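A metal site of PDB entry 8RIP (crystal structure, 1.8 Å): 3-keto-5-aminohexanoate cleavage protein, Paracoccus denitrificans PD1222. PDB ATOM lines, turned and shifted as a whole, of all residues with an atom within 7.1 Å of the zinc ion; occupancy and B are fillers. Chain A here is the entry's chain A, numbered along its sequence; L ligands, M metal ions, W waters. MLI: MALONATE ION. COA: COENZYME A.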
ATOM      1  N   ALA A  36      13.618  35.139  24.620  1.00  0.00           N
ATOM      2  CA  ALA A  36      14.451  33.953  24.456  1.00  0.00           C
ATOM      3  C   ALA A  36      14.746  33.831  22.967  1.00  0.00           C
ATOM      4  O   ALA A  36      13.888  33.408  22.196  1.00  0.00           O
ATOM      5  CB  ALA A  36      13.726  32.724  25.021  1.00  0.00           C
ATOM      6  N   THR A  38      16.813  32.113  20.780  1.00  0.00           N
ATOM      7  CA  THR A  38      17.040  30.993  19.865  1.00  0.00           C
ATOM      8  C   THR A  38      16.847  29.630  20.523  1.00  0.00           C
ATOM      9  O   THR A  38      16.251  28.731  19.913  1.00  0.00           O
ATOM     10  CB  THR A  38      18.444  31.089  19.222  1.00  0.00           C
ATOM     11  OG1 THR A  38      18.559  30.153  18.149  1.00  0.00           O
ATOM     12  CG2 THR A  38      19.582  30.846  20.240  1.00  0.00           C
ATOM     13  N   GLY A  39      17.304  29.452  21.766  1.00  0.00           N
ATOM     14  CA  GLY A  39      17.062  28.181  22.425  1.00  0.00           C
ATOM     15  C   GLY A  39      17.787  27.001  21.783  1.00  0.00           C
ATOM     16  O   GLY A  39      18.788  27.155  21.069  1.00  0.00           O
ATOM     17  N   ALA A  40      17.235  25.811  22.040  1.00  0.00           N
ATOM     18  CA  ALA A  40      17.837  24.552  21.641  1.00  0.00           C
ATOM     19  C   ALA A  40      16.842  23.567  21.040  1.00  0.00           C
ATOM     20  O   ALA A  40      17.255  22.460  20.668  1.00  0.00           O
ATOM     21  CB  ALA A  40      18.531  23.878  22.850  1.00  0.00           C
ATOM     22  N   HIS A  73      17.169  35.896  27.303  1.00  0.00           N
ATOM     23  CA  HIS A  73      17.517  34.516  27.656  1.00  0.00           C
ATOM     24  C   HIS A  73      18.301  33.885  26.509  1.00  0.00           C
ATOM     25  O   HIS A  73      17.843  33.883  25.355  1.00  0.00           O
ATOM     26  CB  HIS A  73      16.258  33.726  27.981  1.00  0.00           C
ATOM     27  CG  HIS A  73      16.476  32.255  28.108  1.00  0.00           C
ATOM     28  ND1 HIS A  73      17.053  31.683  29.213  1.00  0.00           N
ATOM     29  CD2 HIS A  73      16.190  31.229  27.261  1.00  0.00           C
ATOM     30  CE1 HIS A  73      17.119  30.370  29.047  1.00  0.00           C
ATOM     31  NE2 HIS A  73      16.604  30.070  27.875  1.00  0.00           N
ATOM     32  N   LEU A  74      19.485  33.343  26.804  1.00  0.00           N
ATOM     33  CA  LEU A  74      20.487  33.039  25.785  1.00  0.00           C
ATOM     34  C   LEU A  74      20.889  31.557  25.772  1.00  0.00           C
ATOM     35  O   LEU A  74      21.193  30.993  26.818  1.00  0.00           O
ATOM     36  CB  LEU A  74      21.748  33.884  26.012  1.00  0.00           C
ATOM     37  CG  LEU A  74      21.595  35.380  25.716  1.00  0.00           C
ATOM     38  CD1 LEU A  74      22.820  36.148  26.200  1.00  0.00           C
ATOM     39  CD2 LEU A  74      21.418  35.588  24.210  1.00  0.00           C
ATOM     40  N   HIS A  75      20.883  30.972  24.578  1.00  0.00           N
ATOM     41  CA  HIS A  75      21.598  29.756  24.203  1.00  0.00           C
ATOM     42  C   HIS A  75      22.570  30.114  23.084  1.00  0.00           C
ATOM     43  O   HIS A  75      22.462  31.182  22.490  1.00  0.00           O
ATOM     44  CB  HIS A  75      20.657  28.657  23.680  1.00  0.00           C
ATOM     45  CG  HIS A  75      19.654  28.159  24.659  1.00  0.00           C
ATOM     46  ND1 HIS A  75      19.494  26.820  24.941  1.00  0.00           N
ATOM     47  CD2 HIS A  75      18.716  28.809  25.395  1.00  0.00           C
ATOM     48  CE1 HIS A  75      18.506  26.667  25.812  1.00  0.00           C
ATOM     49  NE2 HIS A  75      18.028  27.858  26.112  1.00  0.00           N
ATOM     50  N   THR A 109      21.321  30.095  29.853  1.00  0.00           N
ATOM     51  CA  THR A 109      20.676  28.800  30.085  1.00  0.00           C
ATOM     52  C   THR A 109      21.595  27.869  30.873  1.00  0.00           C
ATOM     53  O   THR A 109      22.805  27.840  30.650  1.00  0.00           O
ATOM     54  CB  THR A 109      20.298  28.149  28.749  1.00  0.00           C
ATOM     55  OG1 THR A 109      19.625  26.916  29.000  1.00  0.00           O
ATOM     56  CG2 THR A 109      21.538  27.875  27.871  1.00  0.00           C
ATOM     57  N   THR A 110      21.017  27.129  31.826  1.00  0.00           N
ATOM     58  CA  THR A 110      21.615  25.890  32.334  1.00  0.00           C
ATOM     59  C   THR A 110      20.836  24.678  31.849  1.00  0.00           C
ATOM     60  O   THR A 110      21.095  23.559  32.311  1.00  0.00           O
ATOM     61  CB  THR A 110      21.698  25.870  33.863  1.00  0.00           C
ATOM     62  OG1 THR A 110      20.397  25.662  34.442  1.00  0.00           O
ATOM     63  CG2 THR A 110      22.319  27.155  34.412  1.00  0.00           C
ATOM     64  N   GLY A 111      19.880  24.874  30.940  1.00  0.00           N
ATOM     65  CA  GLY A 111      19.174  23.764  30.341  1.00  0.00           C
ATOM     66  C   GLY A 111      19.862  23.231  29.098  1.00  0.00           C
ATOM     67  O   GLY A 111      19.816  22.028  28.830  1.00  0.00           O
ATOM     68  N   GLY A 112      20.515  24.116  28.347  1.00  0.00           N
ATOM     69  CA  GLY A 112      21.053  23.704  27.050  1.00  0.00           C
ATOM     70  C   GLY A 112      20.006  22.988  26.239  1.00  0.00           C
ATOM     71  O   GLY A 112      18.833  23.374  26.200  1.00  0.00           O
ATOM     72  N   SER A 134      18.846  30.225  34.011  1.00  0.00           N
ATOM     73  CA  SER A 134      17.689  29.347  34.131  1.00  0.00           C
ATOM     74  C   SER A 134      18.051  28.192  35.060  1.00  0.00           C
ATOM     75  O   SER A 134      19.221  27.821  35.194  1.00  0.00           O
ATOM     76  CB  SER A 134      17.235  28.838  32.761  1.00  0.00           C
ATOM     77  OG  SER A 134      18.220  28.020  32.144  1.00  0.00           O
ATOM     78  N   ASN A 136      16.134  24.462  35.824  1.00  0.00           N
ATOM     79  CA  ASN A 136      15.007  23.591  35.546  1.00  0.00           C
ATOM     80  C   ASN A 136      14.724  22.698  36.743  1.00  0.00           C
ATOM     81  O   ASN A 136      15.651  22.138  37.332  1.00  0.00           O
ATOM     82  CB  ASN A 136      15.304  22.791  34.286  1.00  0.00           C
ATOM     83  CG  ASN A 136      15.451  23.711  33.085  1.00  0.00           C
ATOM     84  OD1 ASN A 136      14.460  24.161  32.515  1.00  0.00           O
ATOM     85  ND2 ASN A 136      16.692  24.066  32.750  1.00  0.00           N
ATOM     86  N   GLU A 193      16.078  31.939  37.337  1.00  0.00           N
ATOM     87  CA  GLU A 193      14.725  31.853  36.831  1.00  0.00           C
ATOM     88  C   GLU A 193      14.336  30.381  36.923  1.00  0.00           C
ATOM     89  O   GLU A 193      14.883  29.544  36.190  1.00  0.00           O
ATOM     90  CB  GLU A 193      14.651  32.343  35.395  1.00  0.00           C
ATOM     91  CG  GLU A 193      13.268  32.215  34.791  1.00  0.00           C
ATOM     92  CD  GLU A 193      13.235  32.758  33.381  1.00  0.00           C
ATOM     93  OE1 GLU A 193      13.856  32.149  32.470  1.00  0.00           O
ATOM     94  OE2 GLU A 193      12.608  33.834  33.211  1.00  0.00           O
ATOM     95  N   GLU A 195      12.475  27.328  36.183  1.00  0.00           N
ATOM     96  CA  GLU A 195      11.620  26.872  35.100  1.00  0.00           C
ATOM     97  C   GLU A 195      10.787  25.692  35.598  1.00  0.00           C
ATOM     98  O   GLU A 195      11.325  24.627  35.905  1.00  0.00           O
ATOM     99  CB  GLU A 195      12.418  26.486  33.857  1.00  0.00           C
ATOM    100  CG  GLU A 195      13.613  27.384  33.558  1.00  0.00           C
ATOM    101  CD  GLU A 195      13.269  28.816  33.227  1.00  0.00           C
ATOM    102  OE1 GLU A 195      14.230  29.622  33.070  1.00  0.00           O
ATOM    103  OE2 GLU A 195      12.070  29.177  33.113  1.00  0.00           O
ATOM    104  N   TYR A 197       7.652  23.277  34.752  1.00  0.00           N
ATOM    105  CA  TYR A 197       6.893  22.746  33.623  1.00  0.00           C
ATOM    106  C   TYR A 197       5.621  22.026  34.040  1.00  0.00           C
ATOM    107  O   TYR A 197       4.868  21.575  33.161  1.00  0.00           O
ATOM    108  CB  TYR A 197       7.770  21.778  32.813  1.00  0.00           C
ATOM    109  CG  TYR A 197       9.050  22.380  32.262  1.00  0.00           C
ATOM    110  CD1 TYR A 197      10.154  22.596  33.084  1.00  0.00           C
ATOM    111  CD2 TYR A 197       9.137  22.732  30.916  1.00  0.00           C
ATOM    112  CE1 TYR A 197      11.335  23.156  32.568  1.00  0.00           C
ATOM    113  CE2 TYR A 197      10.306  23.266  30.385  1.00  0.00           C
ATOM    114  CZ  TYR A 197      11.389  23.480  31.220  1.00  0.00           C
ATOM    115  OH  TYR A 197      12.543  24.027  30.683  1.00  0.00           O
ATOM    116  N   LEU A 257       5.558  31.340  29.897  1.00  0.00           N
ATOM    117  CA  LEU A 257       6.067  30.998  28.544  1.00  0.00           C
ATOM    118  C   LEU A 257       5.018  30.081  27.909  1.00  0.00           C
ATOM    119  O   LEU A 257       4.728  29.049  28.510  1.00  0.00           O
ATOM    120  CB  LEU A 257       7.391  30.266  28.705  1.00  0.00           C
ATOM    121  CG  LEU A 257       8.138  29.779  27.465  1.00  0.00           C
ATOM    122  CD1 LEU A 257       9.455  29.155  27.892  1.00  0.00           C
ATOM    123  CD2 LEU A 257       7.327  28.759  26.681  1.00  0.00           C
ATOM    124  N   ARG A 278       7.296  36.066  28.672  1.00  0.00           N
ATOM    125  CA  ARG A 278       8.438  35.694  27.853  1.00  0.00           C
ATOM    126  C   ARG A 278       7.957  35.457  26.434  1.00  0.00           C
ATOM    127  O   ARG A 278       6.921  34.816  26.221  1.00  0.00           O
ATOM    128  CB  ARG A 278       9.117  34.438  28.417  1.00  0.00           C
ATOM    129  CG  ARG A 278      10.111  33.815  27.476  1.00  0.00           C
ATOM    130  CD  ARG A 278      10.881  32.703  28.205  1.00  0.00           C
ATOM    131  NE  ARG A 278      11.377  31.691  27.281  1.00  0.00           N
ATOM    132  CZ  ARG A 278      12.272  30.767  27.614  1.00  0.00           C
ATOM    133  NH1 ARG A 278      12.871  30.766  28.805  1.00  0.00           N
ATOM    134  NH2 ARG A 278      12.550  29.796  26.750  1.00  0.00           N
ATOM    135  N   GLU A 282      12.950  31.096  20.440  1.00  0.00           N
ATOM    136  CA  GLU A 282      13.191  29.830  21.147  1.00  0.00           C
ATOM    137  C   GLU A 282      11.886  29.076  21.398  1.00  0.00           C
ATOM    138  O   GLU A 282      11.891  27.845  21.455  1.00  0.00           O
ATOM    139  CB  GLU A 282      13.911  30.083  22.470  1.00  0.00           C
ATOM    140  CG  GLU A 282      13.846  28.929  23.470  1.00  0.00           C
ATOM    141  CD  GLU A 282      14.868  29.050  24.596  1.00  0.00           C
ATOM    142  OE1 GLU A 282      15.668  30.002  24.608  1.00  0.00           O
ATOM    143  OE2 GLU A 282      14.875  28.153  25.448  1.00  0.00           O
ATOM    144  N   ASP A 283      10.776  29.799  21.553  1.00  0.00           N
ATOM    145  CA  ASP A 283       9.509  29.226  22.001  1.00  0.00           C
ATOM    146  C   ASP A 283       8.457  29.153  20.906  1.00  0.00           C
ATOM    147  O   ASP A 283       7.605  28.261  20.936  1.00  0.00           O
ATOM    148  CB  ASP A 283       8.932  30.050  23.155  1.00  0.00           C
ATOM    149  CG  ASP A 283       9.878  30.184  24.325  1.00  0.00           C
ATOM    150  OD1 ASP A 283      10.678  29.249  24.554  1.00  0.00           O
ATOM    151  OD2 ASP A 283       9.807  31.224  25.013  1.00  0.00           O
HETATM  152  C1  MLI L   1      14.939  26.326  29.752  1.00  0.00           C
HETATM  153  C2  MLI L   1      16.456  26.534  29.782  1.00  0.00           C
HETATM  154  C3  MLI L   1      14.254  27.646  29.434  1.00  0.00           C
HETATM  155  O6  MLI L   1      17.033  27.080  28.832  1.00  0.00           O
HETATM  156  O7  MLI L   1      17.113  26.123  30.766  1.00  0.00           O
HETATM  157  O8  MLI L   1      14.217  28.049  28.252  1.00  0.00           O
HETATM  158  O9  MLI L   1      13.708  28.317  30.343  1.00  0.00           O
HETATM  159  N1A COA L   2      -2.868  33.985  15.527  1.00  0.00           N
HETATM  160  C2A COA L   2      -3.414  32.990  14.787  1.00  0.00           C
HETATM  161  N3A COA L   2      -2.786  31.939  14.319  1.00  0.00           N
HETATM  162  C4A COA L   2      -1.459  31.821  14.590  1.00  0.00           C
HETATM  163  C5A COA L   2      -0.834  32.808  15.351  1.00  0.00           C
HETATM  164  C6A COA L   2      -1.569  33.893  15.818  1.00  0.00           C
HETATM  165  N6A COA L   2      -0.998  34.862  16.547  1.00  0.00           N
HETATM  166  N7A COA L   2       0.441  32.460  15.464  1.00  0.00           N
HETATM  167  C8A COA L   2       0.597  31.307  14.813  1.00  0.00           C
HETATM  168  N9A COA L   2      -0.547  30.892  14.259  1.00  0.00           N
HETATM  169  C1B COA L   2      -0.929  29.750  13.493  1.00  0.00           C
HETATM  170  C2B COA L   2      -0.031  29.548  12.278  1.00  0.00           C
HETATM  171  O2B COA L   2      -0.632  30.135  11.130  1.00  0.00           O
HETATM  172  C3B COA L   2      -0.002  28.068  12.153  1.00  0.00           C
HETATM  173  O3B COA L   2      -1.272  27.602  11.591  1.00  0.00           O
HETATM  174  P3B COA L   2      -1.347  26.185  10.892  1.00  0.00           P
HETATM  175  O7A COA L   2      -2.731  26.027  10.364  1.00  0.00           O
HETATM  176  O8A COA L   2      -0.312  26.134   9.742  1.00  0.00           O
HETATM  177  O9A COA L   2      -1.051  25.082  11.879  1.00  0.00           O
HETATM  178  C4B COA L   2       0.046  27.631  13.589  1.00  0.00           C
HETATM  179  O4B COA L   2      -0.750  28.605  14.313  1.00  0.00           O
HETATM  180  C5B COA L   2       1.438  27.661  14.122  1.00  0.00           C
HETATM  181  O5B COA L   2       1.335  27.507  15.544  1.00  0.00           O
HETATM  182  P1A COA L   2       1.927  26.101  16.204  1.00  0.00           P
HETATM  183  O1A COA L   2       1.180  24.923  15.644  1.00  0.00           O
HETATM  184  O2A COA L   2       1.776  26.149  17.721  1.00  0.00           O
HETATM  185  O3A COA L   2       3.539  26.065  15.801  1.00  0.00           O
HETATM  186  P2A COA L   2       4.592  24.913  15.274  1.00  0.00           P
HETATM  187  O4A COA L   2       3.817  23.771  14.593  1.00  0.00           O
HETATM  188  O5A COA L   2       5.602  25.534  14.371  1.00  0.00           O
HETATM  189  O6A COA L   2       5.341  24.339  16.623  1.00  0.00           O
HETATM  190  CBP COA L   2       5.421  23.671  18.909  1.00  0.00           C
HETATM  191  CCP COA L   2       4.577  24.290  17.769  1.00  0.00           C
HETATM  192  CDP COA L   2       4.751  23.960  20.207  1.00  0.00           C
HETATM  193  CEP COA L   2       5.525  22.166  18.687  1.00  0.00           C
HETATM  194  CAP COA L   2       6.801  24.290  18.864  1.00  0.00           C
HETATM  195  OAP COA L   2       6.702  25.648  18.540  1.00  0.00           O
HETATM  196  C9P COA L   2       7.485  24.176  20.244  1.00  0.00           C
HETATM  197  O9P COA L   2       7.730  23.077  20.711  1.00  0.00           O
HETATM  198  N8P COA L   2       7.797  25.282  20.895  1.00  0.00           N
HETATM  199  C7P COA L   2       8.462  25.196  22.212  1.00  0.00           C
HETATM  200  C6P COA L   2       9.959  24.909  22.037  1.00  0.00           C
HETATM  201  C5P COA L   2      10.618  24.853  23.394  1.00  0.00           C
HETATM  202  O5P COA L   2      10.470  23.881  24.075  1.00  0.00           O
HETATM  203  N4P COA L   2      11.367  25.860  23.806  1.00  0.00           N
HETATM  204  C3P COA L   2      12.000  25.846  25.109  1.00  0.00           C
HETATM  205  C2P COA L   2      10.888  26.104  26.213  1.00  0.00           C
HETATM  206  S1P COA L   2      11.598  25.933  27.896  1.00  0.00           S
HETATM  207 ZN    ZN M   1      16.131  28.153  27.139  1.00  0.00          ZN
HETATM  208  O   HOH W   1      15.419  25.487  26.858  1.00  0.00           O
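NE of Arg 278 is in salt-bridge range of OD2 of Asp 283. N of Glu 282 lies within hydrogen-bond range of O of Ala 36 (3.1 Å). The side-chain hydroxyl (OG1) of Thr 109 sits close to a ring nitrogen (NE2) of His 75. OE1 of Glu 282 is in salt-bridge range of NH2 of Arg 278 (3.8 Å). N of Gly 39 sits close to OE1 of Glu 282, at 3.3 Å.
The zinc ion is bound by the side-chain carboxylate of Glu 282 (2.1 Å), a ring nitrogen (NE2) of His 73 (2.1 Å), a ring nitrogen (NE2) of His 75 (2.2 Å), an oxygen (O6) of MLI L1 (2.2 Å) and an oxygen (O8) of MLI L1 (2.2 Å). The zinc ion has five donor atoms within binding distance. Slightly farther from the zinc ion lies water W1 (2.8 Å).
Merely in contact with the zinc ion: Arg 278 (3.96 Å). Four residues have an atom within 4 Å of the zinc ion: His 73, His 75, Arg 278 and Glu 282. The nearest printed residue that does not touch the zinc ion is Thr 109 (4.1 Å).
N4P of COA L2 is in hydrogen-bond range of O of Glu 282, 3.1 Å away. S1P of COA L2 lies close to OH of Tyr 197 (3.5 Å). The backbone carbonyl oxygen (O) of Asp 283 sits at hydrogen-bond distance from a nitrogen (N8P) of COA L2.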
